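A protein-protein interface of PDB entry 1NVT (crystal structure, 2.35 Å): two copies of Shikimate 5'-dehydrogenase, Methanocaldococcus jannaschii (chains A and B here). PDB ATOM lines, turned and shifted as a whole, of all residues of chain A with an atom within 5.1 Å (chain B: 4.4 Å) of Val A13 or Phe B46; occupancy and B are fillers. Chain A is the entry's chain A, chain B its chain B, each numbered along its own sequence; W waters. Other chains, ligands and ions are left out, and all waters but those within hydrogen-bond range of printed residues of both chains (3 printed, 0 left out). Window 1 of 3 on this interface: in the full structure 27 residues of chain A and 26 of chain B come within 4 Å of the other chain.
The backbone carbonyl oxygen (O) of Phe B46 lies within hydrogen-bond range of the backbone NH (N) of Gly B18, at 3.3 Å.
The backbone carbonyl oxygen (O) of Val A13 is in hydrogen-bond range of the backbone NH (N) of Val A66 (2.9 Å).
The backbone carbonyl oxygen of Leu B16 sits at hydrogen-bond distance from the backbone NH of Phe B46, 2.6 Å away.
Among the printed residues, merely in contact across the chains: Leu A63 with Phe B46 (3.5 Å), Leu A63 with Asp B47 (3.7 Å) and Val A13 with Phe B46 (3.8 Å).
Of the printed residues of chain B, Val A13 touches Phe B46 (3.8 Å).
Printed residues of chain B within 4 Å of Leu A63: Phe B46 (3.5 Å) and Asp B47 (3.7 Å).
Printed residues of chain A within 4 Å of Phe B46: Val A13 (3.8 Å) and Leu A63 (3.5 Å).
Of the printed residues of chain A, Asp B47 touches Leu A63 (3.7 Å).
The nearest printed residue of chain B that does not touch Val A13 is Val B44 (4.01 Å).
The nearest printed residue of chain A that does not touch Phe B46 is Ile A65 (4.01 Å).
The nearest printed residue of chain A that does not touch Asp B47 is Gly A64 (4.8 Å).
Of the 13 printed residues of chain A, 2 touch a printed residue of chain B.
Hydrophobic or aromatic side chains of chain A within 4 Å of the printed part of chain B: Val A13 and Leu A63.
Along chain A the printed residues that touch a printed residue of chain B span positions 13 to 63.
Of the 12 printed residues of chain B, 2 touch a printed residue of chain A.
Hydrophobic or aromatic side chains of chain B within 4 Å of the printed part of chain A: Phe B46.
Positions printed for both chains: 15, 44, 46 and 65.
Water W2 lies within hydrogen-bond range of the backbone NH of Ala B45 (2.5 Å) and the backbone carbonyl oxygen of Thr A11 (3.1 Å).
Water W1 lies within hydrogen-bond range of N of Asp B47, O of Leu A63 and NZ of Lys A12.
Water W3 bridges the side-chain amino group of Lys A12 (2.9 Å) and the backbone carbonyl oxygen of Ala B45 (3.2 Å).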
ATOM      1  N   THR A  11      23.402 -21.058  16.051  1.00  0.00           N
ATOM      2  CA  THR A  11      23.174 -21.002  14.610  1.00  0.00           C
ATOM      3  C   THR A  11      22.400 -19.738  14.223  1.00  0.00           C
ATOM      4  O   THR A  11      21.400 -19.398  14.868  1.00  0.00           O
ATOM      5  CB  THR A  11      22.364 -22.232  14.125  1.00  0.00           C
ATOM      6  OG1 THR A  11      23.029 -23.443  14.525  1.00  0.00           O
ATOM      7  CG2 THR A  11      22.225 -22.198  12.617  1.00  0.00           C
ATOM      8  N   LYS A  12      22.862 -19.054  13.176  1.00  0.00           N
ATOM      9  CA  LYS A  12      22.218 -17.833  12.683  1.00  0.00           C
ATOM     10  C   LYS A  12      21.267 -18.152  11.521  1.00  0.00           C
ATOM     11  O   LYS A  12      21.542 -19.023  10.684  1.00  0.00           O
ATOM     12  CB  LYS A  12      23.266 -16.807  12.214  1.00  0.00           C
ATOM     13  CG  LYS A  12      24.200 -16.236  13.302  1.00  0.00           C
ATOM     14  CD  LYS A  12      23.465 -15.491  14.419  1.00  0.00           C
ATOM     15  CE  LYS A  12      22.881 -16.444  15.473  1.00  0.00           C
ATOM     16  NZ  LYS A  12      22.225 -15.731  16.623  1.00  0.00           N
ATOM     17  N   VAL A  13      20.157 -17.424  11.468  1.00  0.00           N
ATOM     18  CA  VAL A  13      19.147 -17.650  10.448  1.00  0.00           C
ATOM     19  C   VAL A  13      19.125 -16.628   9.330  1.00  0.00           C
ATOM     20  O   VAL A  13      19.212 -15.417   9.562  1.00  0.00           O
ATOM     21  CB  VAL A  13      17.733 -17.663  11.063  1.00  0.00           C
ATOM     22  CG1 VAL A  13      16.690 -17.932   9.978  1.00  0.00           C
ATOM     23  CG2 VAL A  13      17.659 -18.695  12.165  1.00  0.00           C
ATOM     24  N   ILE A  14      18.992 -17.147   8.116  1.00  0.00           N
ATOM     25  CA  ILE A  14      18.884 -16.347   6.907  1.00  0.00           C
ATOM     26  C   ILE A  14      17.705 -16.982   6.179  1.00  0.00           C
ATOM     27  O   ILE A  14      17.585 -18.206   6.151  1.00  0.00           O
ATOM     28  CB  ILE A  14      20.138 -16.469   6.029  1.00  0.00           C
ATOM     29  CG1 ILE A  14      21.239 -15.561   6.578  1.00  0.00           C
ATOM     30  CG2 ILE A  14      19.801 -16.122   4.598  1.00  0.00           C
ATOM     31  CD1 ILE A  14      22.600 -15.867   6.022  1.00  0.00           C
ATOM     32  N   GLY A  15      16.829 -16.175   5.598  1.00  0.00           N
ATOM     33  CA  GLY A  15      15.698 -16.774   4.913  1.00  0.00           C
ATOM     34  C   GLY A  15      15.281 -16.134   3.610  1.00  0.00           C
ATOM     35  O   GLY A  15      15.724 -15.049   3.260  1.00  0.00           O
ATOM     36  N   VAL A  42      21.931 -21.123   8.764  1.00  0.00           N
ATOM     37  CA  VAL A  42      20.979 -22.022   8.140  1.00  0.00           C
ATOM     38  C   VAL A  42      20.082 -21.167   7.252  1.00  0.00           C
ATOM     39  O   VAL A  42      19.774 -20.010   7.581  1.00  0.00           O
ATOM     40  CB  VAL A  42      20.148 -22.796   9.195  1.00  0.00           C
ATOM     41  CG1 VAL A  42      19.181 -21.865   9.915  1.00  0.00           C
ATOM     42  CG2 VAL A  42      19.405 -23.927   8.522  1.00  0.00           C
ATOM     43  N   VAL A  44      16.410 -20.913   5.352  1.00  0.00           N
ATOM     44  CA  VAL A  44      15.061 -21.462   5.321  1.00  0.00           C
ATOM     45  C   VAL A  44      14.135 -20.620   4.464  1.00  0.00           C
ATOM     46  O   VAL A  44      14.460 -19.490   4.110  1.00  0.00           O
ATOM     47  CB  VAL A  44      14.492 -21.557   6.736  1.00  0.00           C
ATOM     48  CG1 VAL A  44      15.303 -22.565   7.551  1.00  0.00           C
ATOM     49  CG2 VAL A  44      14.559 -20.199   7.400  1.00  0.00           C
ATOM     50  N   PHE A  46      10.455 -18.740   3.940  1.00  0.00           N
ATOM     51  CA  PHE A  46       9.301 -18.187   4.631  1.00  0.00           C
ATOM     52  C   PHE A  46       8.240 -17.721   3.646  1.00  0.00           C
ATOM     53  O   PHE A  46       8.478 -16.808   2.860  1.00  0.00           O
ATOM     54  CB  PHE A  46       9.720 -16.988   5.488  1.00  0.00           C
ATOM     55  CG  PHE A  46      10.684 -17.326   6.589  1.00  0.00           C
ATOM     56  CD1 PHE A  46      11.935 -16.726   6.643  1.00  0.00           C
ATOM     57  CD2 PHE A  46      10.321 -18.206   7.604  1.00  0.00           C
ATOM     58  CE1 PHE A  46      12.812 -16.995   7.700  1.00  0.00           C
ATOM     59  CE2 PHE A  46      11.193 -18.481   8.663  1.00  0.00           C
ATOM     60  CZ  PHE A  46      12.434 -17.874   8.707  1.00  0.00           C
ATOM     61  N   LEU A  63      14.458 -10.687  16.293  1.00  0.00           N
ATOM     62  CA  LEU A  63      14.887 -12.076  16.388  1.00  0.00           C
ATOM     63  C   LEU A  63      16.370 -12.280  16.190  1.00  0.00           C
ATOM     64  O   LEU A  63      16.948 -13.207  16.740  1.00  0.00           O
ATOM     65  CB  LEU A  63      14.123 -12.930  15.365  1.00  0.00           C
ATOM     66  CG  LEU A  63      12.636 -13.110  15.665  1.00  0.00           C
ATOM     67  CD1 LEU A  63      11.926 -13.768  14.490  1.00  0.00           C
ATOM     68  CD2 LEU A  63      12.497 -13.937  16.923  1.00  0.00           C
ATOM     69  N   GLY A  64      16.995 -11.421  15.401  1.00  0.00           N
ATOM     70  CA  GLY A  64      18.413 -11.590  15.181  1.00  0.00           C
ATOM     71  C   GLY A  64      18.653 -12.335  13.888  1.00  0.00           C
ATOM     72  O   GLY A  64      19.729 -12.915  13.675  1.00  0.00           O
ATOM     73  N   ILE A  65      17.637 -12.344  13.031  1.00  0.00           N
ATOM     74  CA  ILE A  65      17.769 -12.989  11.743  1.00  0.00           C
ATOM     75  C   ILE A  65      18.773 -12.104  11.010  1.00  0.00           C
ATOM     76  O   ILE A  65      18.616 -10.879  10.976  1.00  0.00           O
ATOM     77  CB  ILE A  65      16.418 -13.026  11.009  1.00  0.00           C
ATOM     78  CG1 ILE A  65      15.505 -14.053  11.686  1.00  0.00           C
ATOM     79  CG2 ILE A  65      16.629 -13.355   9.547  1.00  0.00           C
ATOM     80  CD1 ILE A  65      14.107 -14.136  11.097  1.00  0.00           C
ATOM     81  N   VAL A  66      19.809 -12.712  10.438  1.00  0.00           N
ATOM     82  CA  VAL A  66      20.852 -11.947   9.768  1.00  0.00           C
ATOM     83  C   VAL A  66      20.509 -11.325   8.426  1.00  0.00           C
ATOM     84  O   VAL A  66      21.037 -10.269   8.091  1.00  0.00           O
ATOM     85  CB  VAL A  66      22.122 -12.796   9.596  1.00  0.00           C
ATOM     86  CG1 VAL A  66      23.265 -11.925   9.079  1.00  0.00           C
ATOM     87  CG2 VAL A  66      22.497 -13.422  10.920  1.00  0.00           C
ATOM     88  N   GLY A  67      19.640 -11.967   7.651  1.00  0.00           N
ATOM     89  CA  GLY A  67      19.284 -11.418   6.353  1.00  0.00           C
ATOM     90  C   GLY A  67      18.240 -12.232   5.615  1.00  0.00           C
ATOM     91  O   GLY A  67      17.715 -13.203   6.149  1.00  0.00           O
ATOM     92  N   GLY B  15      11.357 -21.834  17.160  1.00  0.00           N
ATOM     93  CA  GLY B  15      12.487 -21.243  17.841  1.00  0.00           C
ATOM     94  C   GLY B  15      12.351 -21.054  19.331  1.00  0.00           C
ATOM     95  O   GLY B  15      11.296 -21.243  19.926  1.00  0.00           O
ATOM     96  N   LEU B  16      13.466 -20.686  19.928  1.00  0.00           N
ATOM     97  CA  LEU B  16      13.547 -20.404  21.340  1.00  0.00           C
ATOM     98  C   LEU B  16      13.815 -18.913  21.383  1.00  0.00           C
ATOM     99  O   LEU B  16      14.717 -18.426  20.690  1.00  0.00           O
ATOM    100  CB  LEU B  16      14.738 -21.132  21.970  1.00  0.00           C
ATOM    101  CG  LEU B  16      15.110 -20.646  23.379  1.00  0.00           C
ATOM    102  CD1 LEU B  16      13.981 -21.026  24.354  1.00  0.00           C
ATOM    103  CD2 LEU B  16      16.436 -21.274  23.826  1.00  0.00           C
ATOM    104  N   ILE B  17      13.032 -18.181  22.164  1.00  0.00           N
ATOM    105  CA  ILE B  17      13.272 -16.753  22.292  1.00  0.00           C
ATOM    106  C   ILE B  17      13.664 -16.511  23.745  1.00  0.00           C
ATOM    107  O   ILE B  17      13.083 -17.090  24.671  1.00  0.00           O
ATOM    108  CB  ILE B  17      12.027 -15.898  21.940  1.00  0.00           C
ATOM    109  CG1 ILE B  17      10.836 -16.325  22.781  1.00  0.00           C
ATOM    110  CG2 ILE B  17      11.707 -16.007  20.441  1.00  0.00           C
ATOM    111  CD1 ILE B  17       9.639 -15.410  22.584  1.00  0.00           C
ATOM    112  N   GLY B  18      14.676 -15.677  23.938  1.00  0.00           N
ATOM    113  CA  GLY B  18      15.135 -15.393  25.281  1.00  0.00           C
ATOM    114  C   GLY B  18      16.389 -14.562  25.209  1.00  0.00           C
ATOM    115  O   GLY B  18      16.792 -14.150  24.129  1.00  0.00           O
ATOM    116  N   VAL B  21      20.550 -16.946  24.881  1.00  0.00           N
ATOM    117  CA  VAL B  21      20.051 -18.250  24.472  1.00  0.00           C
ATOM    118  C   VAL B  21      21.166 -19.099  23.884  1.00  0.00           C
ATOM    119  O   VAL B  21      20.942 -20.258  23.515  1.00  0.00           O
ATOM    120  CB  VAL B  21      18.947 -18.141  23.394  1.00  0.00           C
ATOM    121  CG1 VAL B  21      17.763 -17.368  23.930  1.00  0.00           C
ATOM    122  CG2 VAL B  21      19.514 -17.484  22.141  1.00  0.00           C
ATOM    123  N   VAL B  44      15.642 -23.582  16.155  1.00  0.00           N
ATOM    124  CA  VAL B  44      16.770 -22.658  16.286  1.00  0.00           C
ATOM    125  C   VAL B  44      16.578 -21.732  17.490  1.00  0.00           C
ATOM    126  O   VAL B  44      15.498 -21.692  18.081  1.00  0.00           O
ATOM    127  CB  VAL B  44      16.918 -21.795  15.015  1.00  0.00           C
ATOM    128  CG1 VAL B  44      17.163 -22.691  13.795  1.00  0.00           C
ATOM    129  CG2 VAL B  44      15.662 -20.957  14.811  1.00  0.00           C
ATOM    130  N   ALA B  45      17.618 -20.974  17.848  1.00  0.00           N
ATOM    131  CA  ALA B  45      17.535 -20.067  18.995  1.00  0.00           C
ATOM    132  C   ALA B  45      17.629 -18.597  18.597  1.00  0.00           C
ATOM    133  O   ALA B  45      18.501 -18.200  17.823  1.00  0.00           O
ATOM    134  CB  ALA B  45      18.628 -20.408  20.013  1.00  0.00           C
ATOM    135  N   PHE B  46      16.726 -17.785  19.135  1.00  0.00           N
ATOM    136  CA  PHE B  46      16.705 -16.354  18.825  1.00  0.00           C
ATOM    137  C   PHE B  46      17.000 -15.481  20.063  1.00  0.00           C
ATOM    138  O   PHE B  46      16.285 -15.545  21.064  1.00  0.00           O
ATOM    139  CB  PHE B  46      15.338 -15.956  18.254  1.00  0.00           C
ATOM    140  CG  PHE B  46      14.990 -16.614  16.938  1.00  0.00           C
ATOM    141  CD1 PHE B  46      13.935 -17.519  16.853  1.00  0.00           C
ATOM    142  CD2 PHE B  46      15.681 -16.289  15.778  1.00  0.00           C
ATOM    143  CE1 PHE B  46      13.569 -18.087  15.625  1.00  0.00           C
ATOM    144  CE2 PHE B  46      15.324 -16.852  14.549  1.00  0.00           C
ATOM    145  CZ  PHE B  46      14.263 -17.751  14.476  1.00  0.00           C
ATOM    146  N   ASP B  47      18.045 -14.661  19.978  1.00  0.00           N
ATOM    147  CA  ASP B  47      18.426 -13.768  21.077  1.00  0.00           C
ATOM    148  C   ASP B  47      17.599 -12.478  20.960  1.00  0.00           C
ATOM    149  O   ASP B  47      17.880 -11.622  20.119  1.00  0.00           O
ATOM    150  CB  ASP B  47      19.920 -13.457  20.975  1.00  0.00           C
ATOM    151  CG  ASP B  47      20.447 -12.691  22.174  1.00  0.00           C
ATOM    152  OD1 ASP B  47      21.535 -12.089  22.051  1.00  0.00           O
ATOM    153  OD2 ASP B  47      19.791 -12.695  23.237  1.00  0.00           O
ATOM    154  N   VAL B  48      16.584 -12.345  21.811  1.00  0.00           N
ATOM    155  CA  VAL B  48      15.678 -11.193  21.780  1.00  0.00           C
ATOM    156  C   VAL B  48      15.772 -10.272  22.992  1.00  0.00           C
ATOM    157  O   VAL B  48      15.493 -10.699  24.112  1.00  0.00           O
ATOM    158  CB  VAL B  48      14.185 -11.656  21.711  1.00  0.00           C
ATOM    159  CG1 VAL B  48      13.259 -10.443  21.593  1.00  0.00           C
ATOM    160  CG2 VAL B  48      13.976 -12.634  20.561  1.00  0.00           C
ATOM    161  N   ILE B  65       6.504 -18.889  11.224  1.00  0.00           N
ATOM    162  CA  ILE B  65       7.214 -19.630  12.250  1.00  0.00           C
ATOM    163  C   ILE B  65       6.042 -20.247  13.009  1.00  0.00           C
ATOM    164  O   ILE B  65       5.101 -19.543  13.384  1.00  0.00           O
ATOM    165  CB  ILE B  65       8.059 -18.685  13.130  1.00  0.00           C
ATOM    166  CG1 ILE B  65       9.245 -18.177  12.303  1.00  0.00           C
ATOM    167  CG2 ILE B  65       8.554 -19.407  14.367  1.00  0.00           C
ATOM    168  CD1 ILE B  65      10.252 -17.351  13.076  1.00  0.00           C
ATOM    169  N   PHE B  68       7.321 -21.455  19.377  1.00  0.00           N
ATOM    170  CA  PHE B  68       8.480 -21.000  20.129  1.00  0.00           C
ATOM    171  C   PHE B  68       8.445 -21.657  21.493  1.00  0.00           C
ATOM    172  O   PHE B  68       7.425 -22.197  21.913  1.00  0.00           O
ATOM    173  CB  PHE B  68       8.424 -19.506  20.456  1.00  0.00           C
ATOM    174  CG  PHE B  68       8.522 -18.581  19.283  1.00  0.00           C
ATOM    175  CD1 PHE B  68       7.408 -17.861  18.867  1.00  0.00           C
ATOM    176  CD2 PHE B  68       9.745 -18.328  18.680  1.00  0.00           C
ATOM    177  CE1 PHE B  68       7.518 -16.887  17.869  1.00  0.00           C
ATOM    178  CE2 PHE B  68       9.866 -17.360  17.684  1.00  0.00           C
ATOM    179  CZ  PHE B  68       8.755 -16.638  17.280  1.00  0.00           C
HETATM  180  O   HOH W   1      19.421 -14.271  17.690  1.00  0.00           O
HETATM  181  O   HOH W   2      19.919 -21.159  16.884  1.00  0.00           O
HETATM  182  O   HOH W   3      21.549 -17.573  18.696  1.00  0.00           O
